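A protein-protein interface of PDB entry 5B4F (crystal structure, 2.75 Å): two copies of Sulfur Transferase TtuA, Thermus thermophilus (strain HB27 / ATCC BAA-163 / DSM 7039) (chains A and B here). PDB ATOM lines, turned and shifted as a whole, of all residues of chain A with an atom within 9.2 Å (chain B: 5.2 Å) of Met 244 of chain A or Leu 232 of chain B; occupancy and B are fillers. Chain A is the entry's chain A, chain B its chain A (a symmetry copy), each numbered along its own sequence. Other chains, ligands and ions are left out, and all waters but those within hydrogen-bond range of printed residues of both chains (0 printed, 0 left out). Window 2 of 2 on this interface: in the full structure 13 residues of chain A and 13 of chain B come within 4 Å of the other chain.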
ATOM      1  N   ARG A  15     -34.218  18.055   5.192  1.00  0.00           N
ATOM      2  CA  ARG A  15     -34.373  19.453   5.588  1.00  0.00           C
ATOM      3  C   ARG A  15     -34.166  20.372   4.390  1.00  0.00           C
ATOM      4  O   ARG A  15     -34.855  21.373   4.247  1.00  0.00           O
ATOM      5  CB  ARG A  15     -33.411  19.804   6.723  1.00  0.00           C
ATOM      6  CG  ARG A  15     -33.609  18.923   7.959  1.00  0.00           C
ATOM      7  CD  ARG A  15     -32.900  19.478   9.181  1.00  0.00           C
ATOM      8  NE  ARG A  15     -31.474  19.631   8.920  1.00  0.00           N
ATOM      9  CZ  ARG A  15     -30.602  20.197   9.753  1.00  0.00           C
ATOM     10  NH1 ARG A  15     -31.006  20.682  10.923  1.00  0.00           N
ATOM     11  NH2 ARG A  15     -29.320  20.281   9.409  1.00  0.00           N
ATOM     12  N   SER A  16     -33.239  19.986   3.515  1.00  0.00           N
ATOM     13  CA  SER A  16     -32.986  20.655   2.230  1.00  0.00           C
ATOM     14  C   SER A  16     -34.243  20.983   1.448  1.00  0.00           C
ATOM     15  O   SER A  16     -34.266  21.909   0.650  1.00  0.00           O
ATOM     16  CB  SER A  16     -32.104  19.767   1.351  1.00  0.00           C
ATOM     17  OG  SER A  16     -31.073  19.176   2.118  1.00  0.00           O
ATOM     18  N   ARG A  17     -35.278  20.179   1.656  1.00  0.00           N
ATOM     19  CA  ARG A  17     -36.446  20.186   0.799  1.00  0.00           C
ATOM     20  C   ARG A  17     -37.664  20.342   1.699  1.00  0.00           C
ATOM     21  O   ARG A  17     -38.817  20.465   1.230  1.00  0.00           O
ATOM     22  CB  ARG A  17     -36.499  18.890  -0.039  1.00  0.00           C
ATOM     23  CG  ARG A  17     -35.211  18.635  -0.845  1.00  0.00           C
ATOM     24  CD  ARG A  17     -35.182  17.295  -1.549  1.00  0.00           C
ATOM     25  NE  ARG A  17     -35.188  17.436  -3.008  1.00  0.00           N
ATOM     26  CZ  ARG A  17     -34.140  17.216  -3.804  1.00  0.00           C
ATOM     27  NH1 ARG A  17     -32.973  16.837  -3.292  1.00  0.00           N
ATOM     28  NH2 ARG A  17     -34.266  17.369  -5.121  1.00  0.00           N
ATOM     29  N   GLU A 235     -16.459  18.342   2.994  1.00  0.00           N
ATOM     30  CA  GLU A 235     -16.568  18.609   4.420  1.00  0.00           C
ATOM     31  C   GLU A 235     -17.016  20.038   4.654  1.00  0.00           C
ATOM     32  O   GLU A 235     -18.017  20.278   5.329  1.00  0.00           O
ATOM     33  CB  GLU A 235     -15.235  18.375   5.124  1.00  0.00           C
ATOM     34  CG  GLU A 235     -14.697  16.962   5.007  1.00  0.00           C
ATOM     35  CD  GLU A 235     -13.311  16.823   5.624  1.00  0.00           C
ATOM     36  OE1 GLU A 235     -12.956  17.656   6.491  1.00  0.00           O
ATOM     37  OE2 GLU A 235     -12.574  15.888   5.230  1.00  0.00           O
ATOM     38  N   ALA A 236     -16.261  20.974   4.083  1.00  0.00           N
ATOM     39  CA  ALA A 236     -16.481  22.405   4.275  1.00  0.00           C
ATOM     40  C   ALA A 236     -17.902  22.818   3.866  1.00  0.00           C
ATOM     41  O   ALA A 236     -18.559  23.613   4.541  1.00  0.00           O
ATOM     42  CB  ALA A 236     -15.446  23.195   3.488  1.00  0.00           C
ATOM     43  N   LEU A 237     -18.370  22.264   2.755  1.00  0.00           N
ATOM     44  CA  LEU A 237     -19.726  22.513   2.301  1.00  0.00           C
ATOM     45  C   LEU A 237     -20.763  21.819   3.222  1.00  0.00           C
ATOM     46  O   LEU A 237     -21.822  22.374   3.493  1.00  0.00           O
ATOM     47  CB  LEU A 237     -19.891  22.052   0.848  1.00  0.00           C
ATOM     48  CG  LEU A 237     -19.244  22.831  -0.304  1.00  0.00           C
ATOM     49  CD1 LEU A 237     -19.316  22.050  -1.624  1.00  0.00           C
ATOM     50  CD2 LEU A 237     -19.844  24.226  -0.517  1.00  0.00           C
ATOM     51  N   ASN A 238     -20.464  20.621   3.715  1.00  0.00           N
ATOM     52  CA  ASN A 238     -21.380  19.953   4.640  1.00  0.00           C
ATOM     53  C   ASN A 238     -21.455  20.680   5.969  1.00  0.00           C
ATOM     54  O   ASN A 238     -22.516  20.747   6.582  1.00  0.00           O
ATOM     55  CB  ASN A 238     -20.971  18.497   4.874  1.00  0.00           C
ATOM     56  CG  ASN A 238     -21.407  17.585   3.748  1.00  0.00           C
ATOM     57  OD1 ASN A 238     -22.234  17.969   2.899  1.00  0.00           O
ATOM     58  ND2 ASN A 238     -20.859  16.366   3.727  1.00  0.00           N
ATOM     59  N   LEU A 239     -20.322  21.213   6.414  1.00  0.00           N
ATOM     60  CA  LEU A 239     -20.260  22.031   7.623  1.00  0.00           C
ATOM     61  C   LEU A 239     -21.226  23.214   7.520  1.00  0.00           C
ATOM     62  O   LEU A 239     -21.895  23.591   8.495  1.00  0.00           O
ATOM     63  CB  LEU A 239     -18.830  22.519   7.845  1.00  0.00           C
ATOM     64  CG  LEU A 239     -18.474  23.299   9.109  1.00  0.00           C
ATOM     65  CD1 LEU A 239     -18.597  24.789   8.871  1.00  0.00           C
ATOM     66  CD2 LEU A 239     -19.332  22.855  10.276  1.00  0.00           C
ATOM     67  N   VAL A 240     -21.305  23.796   6.330  1.00  0.00           N
ATOM     68  CA  VAL A 240     -22.242  24.878   6.106  1.00  0.00           C
ATOM     69  C   VAL A 240     -23.665  24.318   6.010  1.00  0.00           C
ATOM     70  O   VAL A 240     -24.567  24.827   6.668  1.00  0.00           O
ATOM     71  CB  VAL A 240     -21.876  25.679   4.835  1.00  0.00           C
ATOM     72  CG1 VAL A 240     -22.888  26.778   4.573  1.00  0.00           C
ATOM     73  CG2 VAL A 240     -20.476  26.271   4.970  1.00  0.00           C
ATOM     74  N   GLU A 241     -23.851  23.258   5.218  1.00  0.00           N
ATOM     75  CA  GLU A 241     -25.182  22.698   4.921  1.00  0.00           C
ATOM     76  C   GLU A 241     -25.940  22.271   6.184  1.00  0.00           C
ATOM     77  O   GLU A 241     -27.142  22.519   6.305  1.00  0.00           O
ATOM     78  CB  GLU A 241     -25.049  21.507   3.955  1.00  0.00           C
ATOM     79  CG  GLU A 241     -26.322  20.705   3.664  1.00  0.00           C
ATOM     80  CD  GLU A 241     -27.220  21.355   2.633  1.00  0.00           C
ATOM     81  OE1 GLU A 241     -26.722  22.144   1.789  1.00  0.00           O
ATOM     82  OE2 GLU A 241     -28.440  21.065   2.670  1.00  0.00           O
ATOM     83  N   ARG A 242     -25.223  21.647   7.117  1.00  0.00           N
ATOM     84  CA  ARG A 242     -25.766  21.221   8.408  1.00  0.00           C
ATOM     85  C   ARG A 242     -26.569  22.326   9.095  1.00  0.00           C
ATOM     86  O   ARG A 242     -27.678  22.085   9.553  1.00  0.00           O
ATOM     87  CB  ARG A 242     -24.629  20.755   9.337  1.00  0.00           C
ATOM     88  CG  ARG A 242     -24.747  19.308   9.841  1.00  0.00           C
ATOM     89  CD  ARG A 242     -23.707  18.375   9.218  1.00  0.00           C
ATOM     90  NE  ARG A 242     -22.346  18.662   9.675  1.00  0.00           N
ATOM     91  CZ  ARG A 242     -21.248  18.067   9.207  1.00  0.00           C
ATOM     92  NH1 ARG A 242     -21.335  17.139   8.255  1.00  0.00           N
ATOM     93  NH2 ARG A 242     -20.057  18.408   9.691  1.00  0.00           N
ATOM     94  N   SER A 243     -25.998  23.529   9.140  1.00  0.00           N
ATOM     95  CA  SER A 243     -26.621  24.708   9.745  1.00  0.00           C
ATOM     96  C   SER A 243     -27.545  25.469   8.799  1.00  0.00           C
ATOM     97  O   SER A 243     -28.367  26.268   9.236  1.00  0.00           O
ATOM     98  CB  SER A 243     -25.544  25.672  10.239  1.00  0.00           C
ATOM     99  OG  SER A 243     -24.806  25.095  11.302  1.00  0.00           O
ATOM    100  N   MET A 244     -27.395  25.237   7.502  1.00  0.00           N
ATOM    101  CA  MET A 244     -28.144  25.990   6.504  1.00  0.00           C
ATOM    102  C   MET A 244     -28.580  25.055   5.375  1.00  0.00           C
ATOM    103  O   MET A 244     -28.006  25.068   4.287  1.00  0.00           O
ATOM    104  CB  MET A 244     -27.301  27.161   5.955  1.00  0.00           C
ATOM    105  CG  MET A 244     -26.971  28.245   6.986  1.00  0.00           C
ATOM    106  SD  MET A 244     -25.908  29.566   6.361  1.00  0.00           S
ATOM    107  CE  MET A 244     -26.613  29.789   4.716  1.00  0.00           C
ATOM    108  N   PRO A 245     -29.595  24.226   5.642  1.00  0.00           N
ATOM    109  CA  PRO A 245     -30.085  23.267   4.649  1.00  0.00           C
ATOM    110  C   PRO A 245     -30.400  23.921   3.308  1.00  0.00           C
ATOM    111  O   PRO A 245     -30.986  25.003   3.267  1.00  0.00           O
ATOM    112  CB  PRO A 245     -31.346  22.715   5.310  1.00  0.00           C
ATOM    113  CG  PRO A 245     -31.020  22.778   6.781  1.00  0.00           C
ATOM    114  CD  PRO A 245     -30.306  24.099   6.926  1.00  0.00           C
ATOM    115  N   GLY A 246     -29.983  23.280   2.221  1.00  0.00           N
ATOM    116  CA  GLY A 246     -30.208  23.821   0.898  1.00  0.00           C
ATOM    117  C   GLY A 246     -29.073  24.693   0.405  1.00  0.00           C
ATOM    118  O   GLY A 246     -29.156  25.259  -0.708  1.00  0.00           O
ATOM    119  N   ALA A 247     -28.024  24.819   1.222  1.00  0.00           N
ATOM    120  CA  ALA A 247     -26.862  25.622   0.850  1.00  0.00           C
ATOM    121  C   ALA A 247     -26.230  25.102  -0.433  1.00  0.00           C
ATOM    122  O   ALA A 247     -26.101  25.856  -1.405  1.00  0.00           O
ATOM    123  CB  ALA A 247     -25.847  25.645   1.960  1.00  0.00           C
ATOM    124  N   LYS A 248     -25.866  23.817  -0.448  1.00  0.00           N
ATOM    125  CA  LYS A 248     -25.292  23.215  -1.651  1.00  0.00           C
ATOM    126  C   LYS A 248     -26.144  23.441  -2.891  1.00  0.00           C
ATOM    127  O   LYS A 248     -25.634  23.813  -3.959  1.00  0.00           O
ATOM    128  CB  LYS A 248     -25.107  21.725  -1.487  1.00  0.00           C
ATOM    129  CG  LYS A 248     -24.163  21.297  -0.412  1.00  0.00           C
ATOM    130  CD  LYS A 248     -24.241  19.775  -0.369  1.00  0.00           C
ATOM    131  CE  LYS A 248     -24.011  19.274   1.023  1.00  0.00           C
ATOM    132  NZ  LYS A 248     -24.654  17.960   1.205  1.00  0.00           N
ATOM    133  N   LEU A 249     -27.438  23.183  -2.754  1.00  0.00           N
ATOM    134  CA  LEU A 249     -28.327  23.265  -3.892  1.00  0.00           C
ATOM    135  C   LEU A 249     -28.466  24.728  -4.318  1.00  0.00           C
ATOM    136  O   LEU A 249     -28.449  25.020  -5.506  1.00  0.00           O
ATOM    137  CB  LEU A 249     -29.678  22.616  -3.549  1.00  0.00           C
ATOM    138  CG  LEU A 249     -30.421  21.883  -4.667  1.00  0.00           C
ATOM    139  CD1 LEU A 249     -31.251  20.677  -4.149  1.00  0.00           C
ATOM    140  CD2 LEU A 249     -31.306  22.889  -5.389  1.00  0.00           C
ATOM    141  N   ARG A 250     -28.566  25.648  -3.358  1.00  0.00           N
ATOM    142  CA  ARG A 250     -28.614  27.069  -3.690  1.00  0.00           C
ATOM    143  C   ARG A 250     -27.357  27.466  -4.452  1.00  0.00           C
ATOM    144  O   ARG A 250     -27.431  28.040  -5.540  1.00  0.00           O
ATOM    145  CB  ARG A 250     -28.746  27.935  -2.432  1.00  0.00           C
ATOM    146  CG  ARG A 250     -30.130  27.944  -1.795  1.00  0.00           C
ATOM    147  CD  ARG A 250     -30.318  29.080  -0.808  1.00  0.00           C
ATOM    148  NE  ARG A 250     -29.584  28.877   0.441  1.00  0.00           N
ATOM    149  CZ  ARG A 250     -29.967  28.044   1.400  1.00  0.00           C
ATOM    150  NH1 ARG A 250     -31.071  27.320   1.233  1.00  0.00           N
ATOM    151  NH2 ARG A 250     -29.242  27.928   2.515  1.00  0.00           N
ATOM    152  N   PHE A 251     -26.214  27.146  -3.844  1.00  0.00           N
ATOM    153  CA  PHE A 251     -24.882  27.397  -4.376  1.00  0.00           C
ATOM    154  C   PHE A 251     -24.779  26.988  -5.839  1.00  0.00           C
ATOM    155  O   PHE A 251     -24.501  27.817  -6.724  1.00  0.00           O
ATOM    156  CB  PHE A 251     -23.873  26.635  -3.521  1.00  0.00           C
ATOM    157  CG  PHE A 251     -22.459  26.709  -4.014  1.00  0.00           C
ATOM    158  CD1 PHE A 251     -21.762  25.544  -4.316  1.00  0.00           C
ATOM    159  CD2 PHE A 251     -21.813  27.929  -4.142  1.00  0.00           C
ATOM    160  CE1 PHE A 251     -20.447  25.596  -4.747  1.00  0.00           C
ATOM    161  CE2 PHE A 251     -20.507  27.989  -4.569  1.00  0.00           C
ATOM    162  CZ  PHE A 251     -19.818  26.822  -4.876  1.00  0.00           C
ATOM    163  N   LEU B 171     -23.888  31.112  -1.617  1.00  0.00           N
ATOM    164  CA  LEU B 171     -24.788  30.180  -0.953  1.00  0.00           C
ATOM    165  C   LEU B 171     -26.187  30.788  -0.783  1.00  0.00           C
ATOM    166  O   LEU B 171     -27.197  30.083  -0.844  1.00  0.00           O
ATOM    167  CB  LEU B 171     -24.219  29.770   0.407  1.00  0.00           C
ATOM    168  CG  LEU B 171     -22.779  29.245   0.337  1.00  0.00           C
ATOM    169  CD1 LEU B 171     -22.173  29.010   1.722  1.00  0.00           C
ATOM    170  CD2 LEU B 171     -22.724  27.974  -0.485  1.00  0.00           C
ATOM    171  N   ASN B 172     -26.250  32.097  -0.566  1.00  0.00           N
ATOM    172  CA  ASN B 172     -27.524  32.744  -0.291  1.00  0.00           C
ATOM    173  C   ASN B 172     -27.794  33.935  -1.216  1.00  0.00           C
ATOM    174  O   ASN B 172     -27.857  35.081  -0.768  1.00  0.00           O
ATOM    175  CB  ASN B 172     -27.585  33.202   1.173  1.00  0.00           C
ATOM    176  CG  ASN B 172     -27.626  32.039   2.162  1.00  0.00           C
ATOM    177  OD1 ASN B 172     -27.139  30.948   1.888  1.00  0.00           O
ATOM    178  ND2 ASN B 172     -28.219  32.283   3.331  1.00  0.00           N
ATOM    179  N   ALA B 228     -23.631  33.392  14.265  1.00  0.00           N
ATOM    180  CA  ALA B 228     -23.391  34.295  13.142  1.00  0.00           C
ATOM    181  C   ALA B 228     -23.283  33.497  11.855  1.00  0.00           C
ATOM    182  O   ALA B 228     -22.698  32.415  11.846  1.00  0.00           O
ATOM    183  CB  ALA B 228     -22.116  35.127  13.370  1.00  0.00           C
ATOM    184  N   LYS B 229     -23.862  34.002  10.772  1.00  0.00           N
ATOM    185  CA  LYS B 229     -23.675  33.339   9.490  1.00  0.00           C
ATOM    186  C   LYS B 229     -22.208  33.503   9.074  1.00  0.00           C
ATOM    187  O   LYS B 229     -21.552  32.531   8.679  1.00  0.00           O
ATOM    188  CB  LYS B 229     -24.610  33.906   8.422  1.00  0.00           C
ATOM    189  CG  LYS B 229     -26.049  33.436   8.498  1.00  0.00           C
ATOM    190  CD  LYS B 229     -26.947  34.423   7.749  1.00  0.00           C
ATOM    191  CE  LYS B 229     -27.971  33.713   6.884  1.00  0.00           C
ATOM    192  NZ  LYS B 229     -28.378  34.528   5.698  1.00  0.00           N
ATOM    193  N   SER B 230     -21.703  34.735   9.175  1.00  0.00           N
ATOM    194  CA  SER B 230     -20.313  35.053   8.843  1.00  0.00           C
ATOM    195  C   SER B 230     -19.298  34.085   9.476  1.00  0.00           C
ATOM    196  O   SER B 230     -18.318  33.673   8.837  1.00  0.00           O
ATOM    197  CB  SER B 230     -19.988  36.485   9.268  1.00  0.00           C
ATOM    198  OG  SER B 230     -20.420  36.727  10.599  1.00  0.00           O
ATOM    199  N   LEU B 231     -19.538  33.726  10.733  1.00  0.00           N
ATOM    200  CA  LEU B 231     -18.696  32.767  11.435  1.00  0.00           C
ATOM    201  C   LEU B 231     -18.679  31.373  10.774  1.00  0.00           C
ATOM    202  O   LEU B 231     -17.619  30.771  10.584  1.00  0.00           O
ATOM    203  CB  LEU B 231     -19.157  32.647  12.886  1.00  0.00           C
ATOM    204  CG  LEU B 231     -18.261  33.377  13.882  1.00  0.00           C
ATOM    205  CD1 LEU B 231     -17.978  34.807  13.420  1.00  0.00           C
ATOM    206  CD2 LEU B 231     -18.923  33.357  15.248  1.00  0.00           C
ATOM    207  N   LEU B 232     -19.858  30.867  10.437  1.00  0.00           N
ATOM    208  CA  LEU B 232     -19.996  29.603   9.732  1.00  0.00           C
ATOM    209  C   LEU B 232     -19.171  29.546   8.440  1.00  0.00           C
ATOM    210  O   LEU B 232     -18.543  28.519   8.142  1.00  0.00           O
ATOM    211  CB  LEU B 232     -21.463  29.359   9.406  1.00  0.00           C
ATOM    212  CG  LEU B 232     -21.737  28.044   8.679  1.00  0.00           C
ATOM    213  CD1 LEU B 232     -21.537  26.870   9.628  1.00  0.00           C
ATOM    214  CD2 LEU B 232     -23.139  28.039   8.073  1.00  0.00           C
ATOM    215  N   TYR B 233     -19.190  30.644   7.682  1.00  0.00           N
ATOM    216  CA  TYR B 233     -18.485  30.732   6.409  1.00  0.00           C
ATOM    217  C   TYR B 233     -16.987  30.745   6.621  1.00  0.00           C
ATOM    218  O   TYR B 233     -16.233  30.190   5.823  1.00  0.00           O
ATOM    219  CB  TYR B 233     -18.891  31.991   5.633  1.00  0.00           C
ATOM    220  CG  TYR B 233     -20.373  32.110   5.384  1.00  0.00           C
ATOM    221  CD1 TYR B 233     -21.167  30.980   5.218  1.00  0.00           C
ATOM    222  CD2 TYR B 233     -20.982  33.350   5.314  1.00  0.00           C
ATOM    223  CE1 TYR B 233     -22.529  31.086   4.988  1.00  0.00           C
ATOM    224  CE2 TYR B 233     -22.336  33.465   5.090  1.00  0.00           C
ATOM    225  CZ  TYR B 233     -23.108  32.329   4.923  1.00  0.00           C
ATOM    226  OH  TYR B 233     -24.462  32.433   4.699  1.00  0.00           O
ATOM    227  N   LYS B 234     -16.562  31.400   7.696  1.00  0.00           N
ATOM    228  CA  LYS B 234     -15.145  31.566   7.973  1.00  0.00           C
ATOM    229  C   LYS B 234     -14.527  30.238   8.383  1.00  0.00           C
ATOM    230  O   LYS B 234     -13.417  29.910   7.962  1.00  0.00           O
ATOM    231  CB  LYS B 234     -14.926  32.628   9.050  1.00  0.00           C
ATOM    232  CG  LYS B 234     -15.070  34.040   8.505  1.00  0.00           C
ATOM    233  CD  LYS B 234     -14.743  35.106   9.538  1.00  0.00           C
ATOM    234  CE  LYS B 234     -14.942  36.506   8.947  1.00  0.00           C
ATOM    235  NZ  LYS B 234     -14.758  37.574   9.958  1.00  0.00           N
ATOM    236  N   GLU B 235     -15.249  29.471   9.191  1.00  0.00           N
ATOM    237  CA  GLU B 235     -14.778  28.153   9.583  1.00  0.00           C
ATOM    238  C   GLU B 235     -14.527  27.298   8.358  1.00  0.00           C
ATOM    239  O   GLU B 235     -13.429  26.774   8.173  1.00  0.00           O
ATOM    240  CB  GLU B 235     -15.790  27.457  10.488  1.00  0.00           C
ATOM    241  CG  GLU B 235     -16.094  28.189  11.780  1.00  0.00           C
ATOM    242  CD  GLU B 235     -17.199  27.509  12.580  1.00  0.00           C
ATOM    243  OE1 GLU B 235     -17.421  26.292  12.377  1.00  0.00           O
ATOM    244  OE2 GLU B 235     -17.850  28.196  13.401  1.00  0.00           O
ATOM    245  N   ALA B 236     -15.562  27.171   7.529  1.00  0.00           N
ATOM    246  CA  ALA B 236     -15.539  26.312   6.348  1.00  0.00           C
ATOM    247  C   ALA B 236     -14.388  26.684   5.401  1.00  0.00           C
ATOM    248  O   ALA B 236     -13.707  25.818   4.850  1.00  0.00           O
ATOM    249  CB  ALA B 236     -16.874  26.396   5.624  1.00  0.00           C
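NE of Arg 250 of chain A lies within hydrogen-bond range of O of Leu 171 of chain B, 3.0 Å away.
OH of Tyr 233 of chain B lies close to SD of Met 244 of chain A, 3.6 Å away.
ND2 of Asn 172 of chain B lies close to NZ of Lys 229 of chain B (3.3 Å).
The backbone carbonyl oxygen (O) of Gly 246 of chain A sits close to the guanidinium group (NH1) of Arg 250 of chain A, 3.4 Å away.
NH1 of Arg 250 of chain A sits at hydrogen-bond distance from O of Pro 245 of chain A (3.1 Å).
Ala 236 of chain B touches Ala 236 of chain A (CB to O, 3.4 Å).
CD1 of Leu 232 of chain B touches O of Leu 239 of chain A (3.5 Å).
OE1 of Glu 235 of chain B touches CD1 of Leu 239 of chain A (3.99 Å).
Leu 171 of chain B touches Val 240 of chain A (CD1 to CG1, 3.7 Å).
CG1 of Val 240 of chain A touches CD2 of Leu 232 of chain B (3.7 Å).
Val 240 of chain A touches Ala 236 of chain B.
Met 244 of chain A touches Asn 172 of chain B.
Leu 232 of chain B touches Met 244 of chain A (CD2 to SD, 3.6 Å).
Arg 250 of chain A touches Asn 172 of chain B.
Leu 171 of chain B touches Phe 251 of chain A.
Printed residues of chain B within 4 Å of Leu 239 of chain A: Leu 232 (3.5 Å) and Glu 235 (3.99 Å).
Of chain B, only Asn 172 (3.1 Å), Leu 232 (3.6 Å) and Tyr 233 (3.4 Å) come within 4 Å of Met 244 of chain A.
Of the printed residues of chain A, Ala 236 of chain B touches Ala 236 (3.4 Å) and Val 240 (3.7 Å).
The nearest residue of chain B that does not touch Met 244 of chain A is Lys 229 of chain B (4.4 Å).
The nearest printed residue of chain B that does not touch Leu 239 of chain A is Ala 236 of chain B (4.01 Å).
Printed residues of chain B that touch a printed residue of chain A: Leu 171, Asn 172, Leu 232, Tyr 233, Glu 235 and Ala 236.
Hydrophobic or aromatic side chains of chain B that line the printed part of chain A: Leu 171, Leu 232, Tyr 233 and Ala 236.
Of the 20 printed residues of chain A, 6 touch a printed residue of chain B.
Ala 236 of chain B touches its own counterpart, Ala 236 of chain A.
Of the 12 pairs that touch across the chains among the printed residues, 1 has its exchanged pair printed and touching as well.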
